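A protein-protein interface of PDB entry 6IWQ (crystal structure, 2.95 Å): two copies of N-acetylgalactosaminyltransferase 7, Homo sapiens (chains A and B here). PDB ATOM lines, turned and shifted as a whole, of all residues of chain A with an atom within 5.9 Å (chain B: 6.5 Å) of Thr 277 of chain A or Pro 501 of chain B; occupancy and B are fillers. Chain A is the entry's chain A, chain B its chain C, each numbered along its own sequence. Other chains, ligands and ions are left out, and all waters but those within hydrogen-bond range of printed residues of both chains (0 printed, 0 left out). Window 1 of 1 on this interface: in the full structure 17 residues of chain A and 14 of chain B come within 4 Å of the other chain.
Thr 277 of chain A touches just one residue of chain B: Pro 501 (3.6 Å).
Of the printed residues of chain B, Glu 279 of chain A touches Pro 501 (3.9 Å) and His 573 (2.9 Å).
Leu 499 of chain B touches none of the printed residues of chain A.
Printed residues of chain A within 4 Å of His 573 of chain B: Glu 279.
OE2 of Glu 279 of chain A sits at hydrogen-bond distance from NE2 of His 573 of chain B, 2.9 Å away.
Among the printed residues, merely in contact across the chains: Pro 95 of chain A with Pro 501 of chain B (3.8 Å), Val 97 of chain A with Pro 501 of chain B (3.9 Å), Val 97 of chain A with Cys 502 of chain B (3.6 Å), Val 97 of chain A with His 503 of chain B (3.9 Å), Thr 277 of chain A with Pro 501 of chain B (3.6 Å) and Glu 279 of chain A with Pro 501 of chain B (3.9 Å).
Of the 14 printed residues of chain A, 4 touch a printed residue of chain B.
Printed residues of chain A that touch a printed residue of chain B: Pro 95, Val 97, Thr 277 and Glu 279.
Hydrophobic or aromatic side chains of chain A that line the printed part of chain B: Pro 95 and Val 97.
Among the printed residues, 7 pairs touch across the chains.
No position is printed for both chains.
Of the 7 pairs that touch across the chains among the printed residues, none has its exchanged pair printed and touching as well.
SG of Cys 485 of chain B forms a disulfide with SG of Cys 502 of chain B, at 2.0 Å.
The backbone carbonyl oxygen (O) of Thr 277 of chain A lies within hydrogen-bond range of the backbone NH (N) of Leu 96 of chain A, at 2.9 Å.
N of Tyr 484 of chain B sits close to SG of Cys 502 of chain B (3.8 Å).
The side-chain hydroxyl (OG1) of Thr 277 of chain A lies within hydrogen-bond range of the side-chain carboxylate (OE1) of Glu 279 of chain A (2.6 Å).
The backbone carbonyl oxygen of Pro 501 of chain B is in hydrogen-bond range of the side-chain amide nitrogen of Gln 509 of chain B, at 3.1 Å.
The backbone NH (N) of Thr 277 of chain A lies within hydrogen-bond range of the side-chain amide oxygen (OD1) of Asn 274 of chain A, 3.1 Å away.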
ATOM      1  N   LYS A  94      16.326 -11.809 -21.055  1.00  0.00           N
ATOM      2  CA  LYS A  94      15.191 -10.928 -20.916  1.00  0.00           C
ATOM      3  C   LYS A  94      15.517  -9.656 -21.643  1.00  0.00           C
ATOM      4  O   LYS A  94      16.663  -9.251 -21.662  1.00  0.00           O
ATOM      5  CB  LYS A  94      14.987 -10.610 -19.442  1.00  0.00           C
ATOM      6  CG  LYS A  94      13.542 -10.540 -18.996  1.00  0.00           C
ATOM      7  CD  LYS A  94      13.327  -9.407 -18.012  1.00  0.00           C
ATOM      8  CE  LYS A  94      13.177  -9.929 -16.597  1.00  0.00           C
ATOM      9  NZ  LYS A  94      12.897  -8.839 -15.624  1.00  0.00           N
ATOM     10  N   PRO A  95      14.539  -9.010 -22.258  1.00  0.00           N
ATOM     11  CA  PRO A  95      14.872  -7.698 -22.824  1.00  0.00           C
ATOM     12  C   PRO A  95      15.161  -6.647 -21.766  1.00  0.00           C
ATOM     13  O   PRO A  95      14.511  -6.625 -20.734  1.00  0.00           O
ATOM     14  CB  PRO A  95      13.632  -7.320 -23.623  1.00  0.00           C
ATOM     15  CG  PRO A  95      12.526  -7.976 -22.933  1.00  0.00           C
ATOM     16  CD  PRO A  95      13.090  -9.317 -22.697  1.00  0.00           C
ATOM     17  N   LEU A  96      16.130  -5.780 -22.034  1.00  0.00           N
ATOM     18  CA  LEU A  96      16.460  -4.704 -21.125  1.00  0.00           C
ATOM     19  C   LEU A  96      15.871  -3.440 -21.680  1.00  0.00           C
ATOM     20  O   LEU A  96      16.308  -2.941 -22.693  1.00  0.00           O
ATOM     21  CB  LEU A  96      17.966  -4.536 -21.058  1.00  0.00           C
ATOM     22  CG  LEU A  96      18.615  -4.090 -19.761  1.00  0.00           C
ATOM     23  CD1 LEU A  96      20.086  -3.850 -19.998  1.00  0.00           C
ATOM     24  CD2 LEU A  96      17.973  -2.847 -19.193  1.00  0.00           C
ATOM     25  N   VAL A  97      14.892  -2.896 -20.984  1.00  0.00           N
ATOM     26  CA  VAL A  97      14.206  -1.704 -21.465  1.00  0.00           C
ATOM     27  C   VAL A  97      14.534  -0.569 -20.503  1.00  0.00           C
ATOM     28  O   VAL A  97      14.234  -0.661 -19.306  1.00  0.00           O
ATOM     29  CB  VAL A  97      12.686  -1.937 -21.582  1.00  0.00           C
ATOM     30  CG1 VAL A  97      12.013  -0.702 -22.065  1.00  0.00           C
ATOM     31  CG2 VAL A  97      12.379  -3.076 -22.554  1.00  0.00           C
ATOM     32  N   ASN A 116      22.755  -0.027 -29.197  1.00  0.00           N
ATOM     33  CA  ASN A 116      22.517   0.583 -27.901  1.00  0.00           C
ATOM     34  C   ASN A 116      23.648   0.210 -26.935  1.00  0.00           C
ATOM     35  O   ASN A 116      23.503  -0.737 -26.160  1.00  0.00           O
ATOM     36  CB  ASN A 116      21.158   0.132 -27.374  1.00  0.00           C
ATOM     37  CG  ASN A 116      20.743   0.873 -26.146  1.00  0.00           C
ATOM     38  OD1 ASN A 116      19.589   0.776 -25.700  1.00  0.00           O
ATOM     39  ND2 ASN A 116      21.665   1.663 -25.602  1.00  0.00           N
ATOM     40  N   ALA A 119      22.882   0.068 -23.010  1.00  0.00           N
ATOM     41  CA  ALA A 119      22.215  -1.145 -22.555  1.00  0.00           C
ATOM     42  C   ALA A 119      23.179  -2.315 -22.539  1.00  0.00           C
ATOM     43  O   ALA A 119      23.253  -3.052 -21.556  1.00  0.00           O
ATOM     44  CB  ALA A 119      21.013  -1.455 -23.444  1.00  0.00           C
ATOM     45  N   ILE A 123      24.834  -5.161 -19.283  1.00  0.00           N
ATOM     46  CA  ILE A 123      24.579  -6.599 -19.301  1.00  0.00           C
ATOM     47  C   ILE A 123      25.895  -7.333 -19.106  1.00  0.00           C
ATOM     48  O   ILE A 123      26.930  -6.938 -19.653  1.00  0.00           O
ATOM     49  CB  ILE A 123      23.902  -7.022 -20.615  1.00  0.00           C
ATOM     50  CG1 ILE A 123      22.689  -6.141 -20.904  1.00  0.00           C
ATOM     51  CG2 ILE A 123      23.479  -8.487 -20.558  1.00  0.00           C
ATOM     52  CD1 ILE A 123      21.947  -6.511 -22.190  1.00  0.00           C
ATOM     53  N   ARG A 127      26.671 -13.346 -19.349  1.00  0.00           N
ATOM     54  CA  ARG A 127      25.286 -13.566 -19.119  1.00  0.00           C
ATOM     55  C   ARG A 127      24.827 -14.859 -19.647  1.00  0.00           C
ATOM     56  O   ARG A 127      25.498 -15.452 -20.387  1.00  0.00           O
ATOM     57  CB  ARG A 127      24.469 -12.403 -19.668  1.00  0.00           C
ATOM     58  CG  ARG A 127      23.744 -12.587 -20.964  1.00  0.00           C
ATOM     59  CD  ARG A 127      23.568 -11.286 -21.663  1.00  0.00           C
ATOM     60  NE  ARG A 127      23.103 -11.440 -23.019  1.00  0.00           N
ATOM     61  CZ  ARG A 127      21.896 -11.120 -23.411  1.00  0.00           C
ATOM     62  NH1 ARG A 127      21.570 -11.272 -24.639  1.00  0.00           N
ATOM     63  NH2 ARG A 127      21.016 -10.659 -22.585  1.00  0.00           N
ATOM     64  N   ASN A 274      18.492  -8.491 -30.602  1.00  0.00           N
ATOM     65  CA  ASN A 274      18.005  -7.126 -30.718  1.00  0.00           C
ATOM     66  C   ASN A 274      19.085  -6.144 -30.307  1.00  0.00           C
ATOM     67  O   ASN A 274      19.566  -6.176 -29.176  1.00  0.00           O
ATOM     68  CB  ASN A 274      16.766  -6.936 -29.858  1.00  0.00           C
ATOM     69  CG  ASN A 274      16.200  -5.543 -29.975  1.00  0.00           C
ATOM     70  OD1 ASN A 274      16.942  -4.561 -30.026  1.00  0.00           O
ATOM     71  ND2 ASN A 274      14.873  -5.444 -30.053  1.00  0.00           N
ATOM     72  N   GLY A 275      19.441  -5.246 -31.224  1.00  0.00           N
ATOM     73  CA  GLY A 275      20.470  -4.249 -30.980  1.00  0.00           C
ATOM     74  C   GLY A 275      20.108  -3.163 -29.992  1.00  0.00           C
ATOM     75  O   GLY A 275      20.922  -2.265 -29.758  1.00  0.00           O
ATOM     76  N   ASN A 276      18.924  -3.220 -29.414  1.00  0.00           N
ATOM     77  CA  ASN A 276      18.471  -2.204 -28.485  1.00  0.00           C
ATOM     78  C   ASN A 276      18.071  -2.750 -27.115  1.00  0.00           C
ATOM     79  O   ASN A 276      18.311  -2.086 -26.102  1.00  0.00           O
ATOM     80  CB  ASN A 276      17.291  -1.457 -29.102  1.00  0.00           C
ATOM     81  CG  ASN A 276      16.740  -0.431 -28.190  1.00  0.00           C
ATOM     82  OD1 ASN A 276      17.479   0.375 -27.637  1.00  0.00           O
ATOM     83  ND2 ASN A 276      15.436  -0.475 -27.976  1.00  0.00           N
ATOM     84  N   THR A 277      17.493  -3.951 -27.050  1.00  0.00           N
ATOM     85  CA  THR A 277      17.091  -4.566 -25.791  1.00  0.00           C
ATOM     86  C   THR A 277      17.692  -5.959 -25.551  1.00  0.00           C
ATOM     87  O   THR A 277      17.499  -6.527 -24.470  1.00  0.00           O
ATOM     88  CB  THR A 277      15.570  -4.631 -25.757  1.00  0.00           C
ATOM     89  OG1 THR A 277      15.129  -5.292 -26.951  1.00  0.00           O
ATOM     90  CG2 THR A 277      15.084  -3.248 -25.816  1.00  0.00           C
ATOM     91  N   TYR A 278      18.366  -6.537 -26.543  1.00  0.00           N
ATOM     92  CA  TYR A 278      19.275  -7.669 -26.458  1.00  0.00           C
ATOM     93  C   TYR A 278      18.608  -8.975 -26.103  1.00  0.00           C
ATOM     94  O   TYR A 278      19.307  -9.920 -25.767  1.00  0.00           O
ATOM     95  CB  TYR A 278      20.410  -7.401 -25.477  1.00  0.00           C
ATOM     96  CG  TYR A 278      21.294  -6.316 -25.975  1.00  0.00           C
ATOM     97  CD1 TYR A 278      20.998  -4.982 -25.729  1.00  0.00           C
ATOM     98  CD2 TYR A 278      22.401  -6.618 -26.742  1.00  0.00           C
ATOM     99  CE1 TYR A 278      21.808  -3.977 -26.221  1.00  0.00           C
ATOM    100  CE2 TYR A 278      23.216  -5.632 -27.231  1.00  0.00           C
ATOM    101  CZ  TYR A 278      22.920  -4.317 -26.974  1.00  0.00           C
ATOM    102  OH  TYR A 278      23.769  -3.370 -27.478  1.00  0.00           O
ATOM    103  N   GLU A 279      17.287  -9.070 -26.172  1.00  0.00           N
ATOM    104  CA  GLU A 279      16.673 -10.387 -26.174  1.00  0.00           C
ATOM    105  C   GLU A 279      16.938 -11.063 -27.521  1.00  0.00           C
ATOM    106  O   GLU A 279      17.227 -10.401 -28.515  1.00  0.00           O
ATOM    107  CB  GLU A 279      15.181 -10.287 -25.910  1.00  0.00           C
ATOM    108  CG  GLU A 279      14.362 -10.166 -27.146  1.00  0.00           C
ATOM    109  CD  GLU A 279      14.310  -8.759 -27.616  1.00  0.00           C
ATOM    110  OE1 GLU A 279      14.966  -7.905 -26.983  1.00  0.00           O
ATOM    111  OE2 GLU A 279      13.592  -8.501 -28.605  1.00  0.00           O
ATOM    112  N   ALA B 483       4.847  -8.340 -21.308  1.00  0.00           N
ATOM    113  CA  ALA B 483       5.529  -7.080 -21.548  1.00  0.00           C
ATOM    114  C   ALA B 483       5.901  -6.966 -23.013  1.00  0.00           C
ATOM    115  O   ALA B 483       6.956  -6.445 -23.359  1.00  0.00           O
ATOM    116  CB  ALA B 483       6.768  -6.955 -20.671  1.00  0.00           C
ATOM    117  N   TYR B 484       5.063  -7.476 -23.900  1.00  0.00           N
ATOM    118  CA  TYR B 484       5.292  -7.324 -25.324  1.00  0.00           C
ATOM    119  C   TYR B 484       4.157  -6.499 -25.883  1.00  0.00           C
ATOM    120  O   TYR B 484       3.031  -6.590 -25.398  1.00  0.00           O
ATOM    121  CB  TYR B 484       5.398  -8.671 -26.028  1.00  0.00           C
ATOM    122  CG  TYR B 484       6.622  -9.445 -25.605  1.00  0.00           C
ATOM    123  CD1 TYR B 484       7.892  -9.110 -26.086  1.00  0.00           C
ATOM    124  CD2 TYR B 484       6.522 -10.488 -24.709  1.00  0.00           C
ATOM    125  CE1 TYR B 484       9.022  -9.805 -25.691  1.00  0.00           C
ATOM    126  CE2 TYR B 484       7.645 -11.197 -24.307  1.00  0.00           C
ATOM    127  CZ  TYR B 484       8.897 -10.853 -24.801  1.00  0.00           C
ATOM    128  OH  TYR B 484      10.025 -11.555 -24.410  1.00  0.00           O
ATOM    129  N   CYS B 485       4.488  -5.641 -26.852  1.00  0.00           N
ATOM    130  CA  CYS B 485       3.564  -4.695 -27.477  1.00  0.00           C
ATOM    131  C   CYS B 485       3.669  -4.834 -28.985  1.00  0.00           C
ATOM    132  O   CYS B 485       4.762  -5.030 -29.522  1.00  0.00           O
ATOM    133  CB  CYS B 485       3.880  -3.230 -27.122  1.00  0.00           C
ATOM    134  SG  CYS B 485       3.335  -2.597 -25.495  1.00  0.00           S
ATOM    135  N   ASP B 487       4.384  -3.387 -32.159  1.00  0.00           N
ATOM    136  CA  ASP B 487       5.257  -2.276 -32.463  1.00  0.00           C
ATOM    137  C   ASP B 487       5.327  -2.111 -33.967  1.00  0.00           C
ATOM    138  O   ASP B 487       5.563  -3.056 -34.696  1.00  0.00           O
ATOM    139  CB  ASP B 487       6.632  -2.531 -31.859  1.00  0.00           C
ATOM    140  CG  ASP B 487       7.683  -1.640 -32.417  1.00  0.00           C
ATOM    141  OD1 ASP B 487       7.548  -0.420 -32.331  1.00  0.00           O
ATOM    142  OD2 ASP B 487       8.670  -2.163 -32.938  1.00  0.00           O
ATOM    143  N   LEU B 499       5.970  -7.592 -33.102  1.00  0.00           N
ATOM    144  CA  LEU B 499       5.882  -7.507 -31.659  1.00  0.00           C
ATOM    145  C   LEU B 499       7.236  -7.044 -31.136  1.00  0.00           C
ATOM    146  O   LEU B 499       8.265  -7.267 -31.778  1.00  0.00           O
ATOM    147  CB  LEU B 499       5.491  -8.865 -31.066  1.00  0.00           C
ATOM    148  CG  LEU B 499       4.971  -8.928 -29.627  1.00  0.00           C
ATOM    149  CD1 LEU B 499       3.546  -8.419 -29.549  1.00  0.00           C
ATOM    150  CD2 LEU B 499       5.079 -10.334 -29.044  1.00  0.00           C
ATOM    151  N   GLY B 500       7.243  -6.367 -29.993  1.00  0.00           N
ATOM    152  CA  GLY B 500       8.485  -5.961 -29.381  1.00  0.00           C
ATOM    153  C   GLY B 500       8.310  -5.693 -27.905  1.00  0.00           C
ATOM    154  O   GLY B 500       7.178  -5.613 -27.406  1.00  0.00           O
ATOM    155  N   PRO B 501       9.413  -5.581 -27.168  1.00  0.00           N
ATOM    156  CA  PRO B 501       9.312  -5.297 -25.727  1.00  0.00           C
ATOM    157  C   PRO B 501       8.711  -3.922 -25.491  1.00  0.00           C
ATOM    158  O   PRO B 501       9.144  -2.935 -26.083  1.00  0.00           O
ATOM    159  CB  PRO B 501      10.763  -5.385 -25.237  1.00  0.00           C
ATOM    160  CG  PRO B 501      11.602  -5.522 -26.474  1.00  0.00           C
ATOM    161  CD  PRO B 501      10.746  -6.054 -27.557  1.00  0.00           C
ATOM    162  N   CYS B 502       7.691  -3.874 -24.635  1.00  0.00           N
ATOM    163  CA  CYS B 502       6.988  -2.625 -24.345  1.00  0.00           C
ATOM    164  C   CYS B 502       7.917  -1.627 -23.668  1.00  0.00           C
ATOM    165  O   CYS B 502       8.693  -1.982 -22.772  1.00  0.00           O
ATOM    166  CB  CYS B 502       5.759  -2.863 -23.451  1.00  0.00           C
ATOM    167  SG  CYS B 502       4.327  -3.795 -24.167  1.00  0.00           S
ATOM    168  N   HIS B 503       7.831  -0.384 -24.109  1.00  0.00           N
ATOM    169  CA  HIS B 503       8.551   0.706 -23.487  1.00  0.00           C
ATOM    170  C   HIS B 503       7.694   1.845 -22.965  1.00  0.00           C
ATOM    171  O   HIS B 503       8.174   2.682 -22.246  1.00  0.00           O
ATOM    172  CB  HIS B 503       9.583   1.253 -24.442  1.00  0.00           C
ATOM    173  CG  HIS B 503       9.004   1.758 -25.714  1.00  0.00           C
ATOM    174  ND1 HIS B 503       8.122   2.805 -25.755  1.00  0.00           N
ATOM    175  CD2 HIS B 503       9.183   1.365 -26.988  1.00  0.00           C
ATOM    176  CE1 HIS B 503       7.778   3.034 -27.003  1.00  0.00           C
ATOM    177  NE2 HIS B 503       8.408   2.173 -27.770  1.00  0.00           N
ATOM    178  N   ARG B 504       6.430   1.870 -23.337  1.00  0.00           N
ATOM    179  CA  ARG B 504       5.483   2.822 -22.802  1.00  0.00           C
ATOM    180  C   ARG B 504       5.825   4.223 -23.183  1.00  0.00           C
ATOM    181  O   ARG B 504       5.405   5.151 -22.537  1.00  0.00           O
ATOM    182  CB  ARG B 504       5.443   2.725 -21.302  1.00  0.00           C
ATOM    183  CG  ARG B 504       4.388   1.786 -20.769  1.00  0.00           C
ATOM    184  CD  ARG B 504       4.424   1.737 -19.261  1.00  0.00           C
ATOM    185  NE  ARG B 504       3.830   0.505 -18.775  1.00  0.00           N
ATOM    186  CZ  ARG B 504       3.970   0.041 -17.538  1.00  0.00           C
ATOM    187  NH1 ARG B 504       4.685   0.722 -16.656  1.00  0.00           N
ATOM    188  NH2 ARG B 504       3.390  -1.100 -17.174  1.00  0.00           N
ATOM    189  N   GLN B 509       4.705   2.291 -30.765  1.00  0.00           N
ATOM    190  CA  GLN B 509       3.898   1.341 -30.003  1.00  0.00           C
ATOM    191  C   GLN B 509       2.591   1.957 -29.540  1.00  0.00           C
ATOM    192  O   GLN B 509       2.046   1.533 -28.522  1.00  0.00           O
ATOM    193  CB  GLN B 509       4.641   0.800 -28.780  1.00  0.00           C
ATOM    194  CG  GLN B 509       6.004   0.199 -29.059  1.00  0.00           C
ATOM    195  CD  GLN B 509       6.566  -0.606 -27.902  1.00  0.00           C
ATOM    196  OE1 GLN B 509       6.208  -0.410 -26.725  1.00  0.00           O
ATOM    197  NE2 GLN B 509       7.479  -1.501 -28.224  1.00  0.00           N
ATOM    198  N   HIS B 573       9.094 -12.798 -32.617  1.00  0.00           N
ATOM    199  CA  HIS B 573       8.198 -11.727 -32.264  1.00  0.00           C
ATOM    200  C   HIS B 573       7.355 -11.486 -33.476  1.00  0.00           C
ATOM    201  O   HIS B 573       7.791 -10.845 -34.421  1.00  0.00           O
ATOM    202  CB  HIS B 573       8.992 -10.459 -32.029  1.00  0.00           C
ATOM    203  CG  HIS B 573       9.824 -10.479 -30.794  1.00  0.00           C
ATOM    204  ND1 HIS B 573       9.797 -11.517 -29.895  1.00  0.00           N
ATOM    205  CD2 HIS B 573      10.700  -9.578 -30.305  1.00  0.00           C
ATOM    206  CE1 HIS B 573      10.622 -11.255 -28.901  1.00  0.00           C
ATOM    207  NE2 HIS B 573      11.181 -10.084 -29.126  1.00  0.00           N
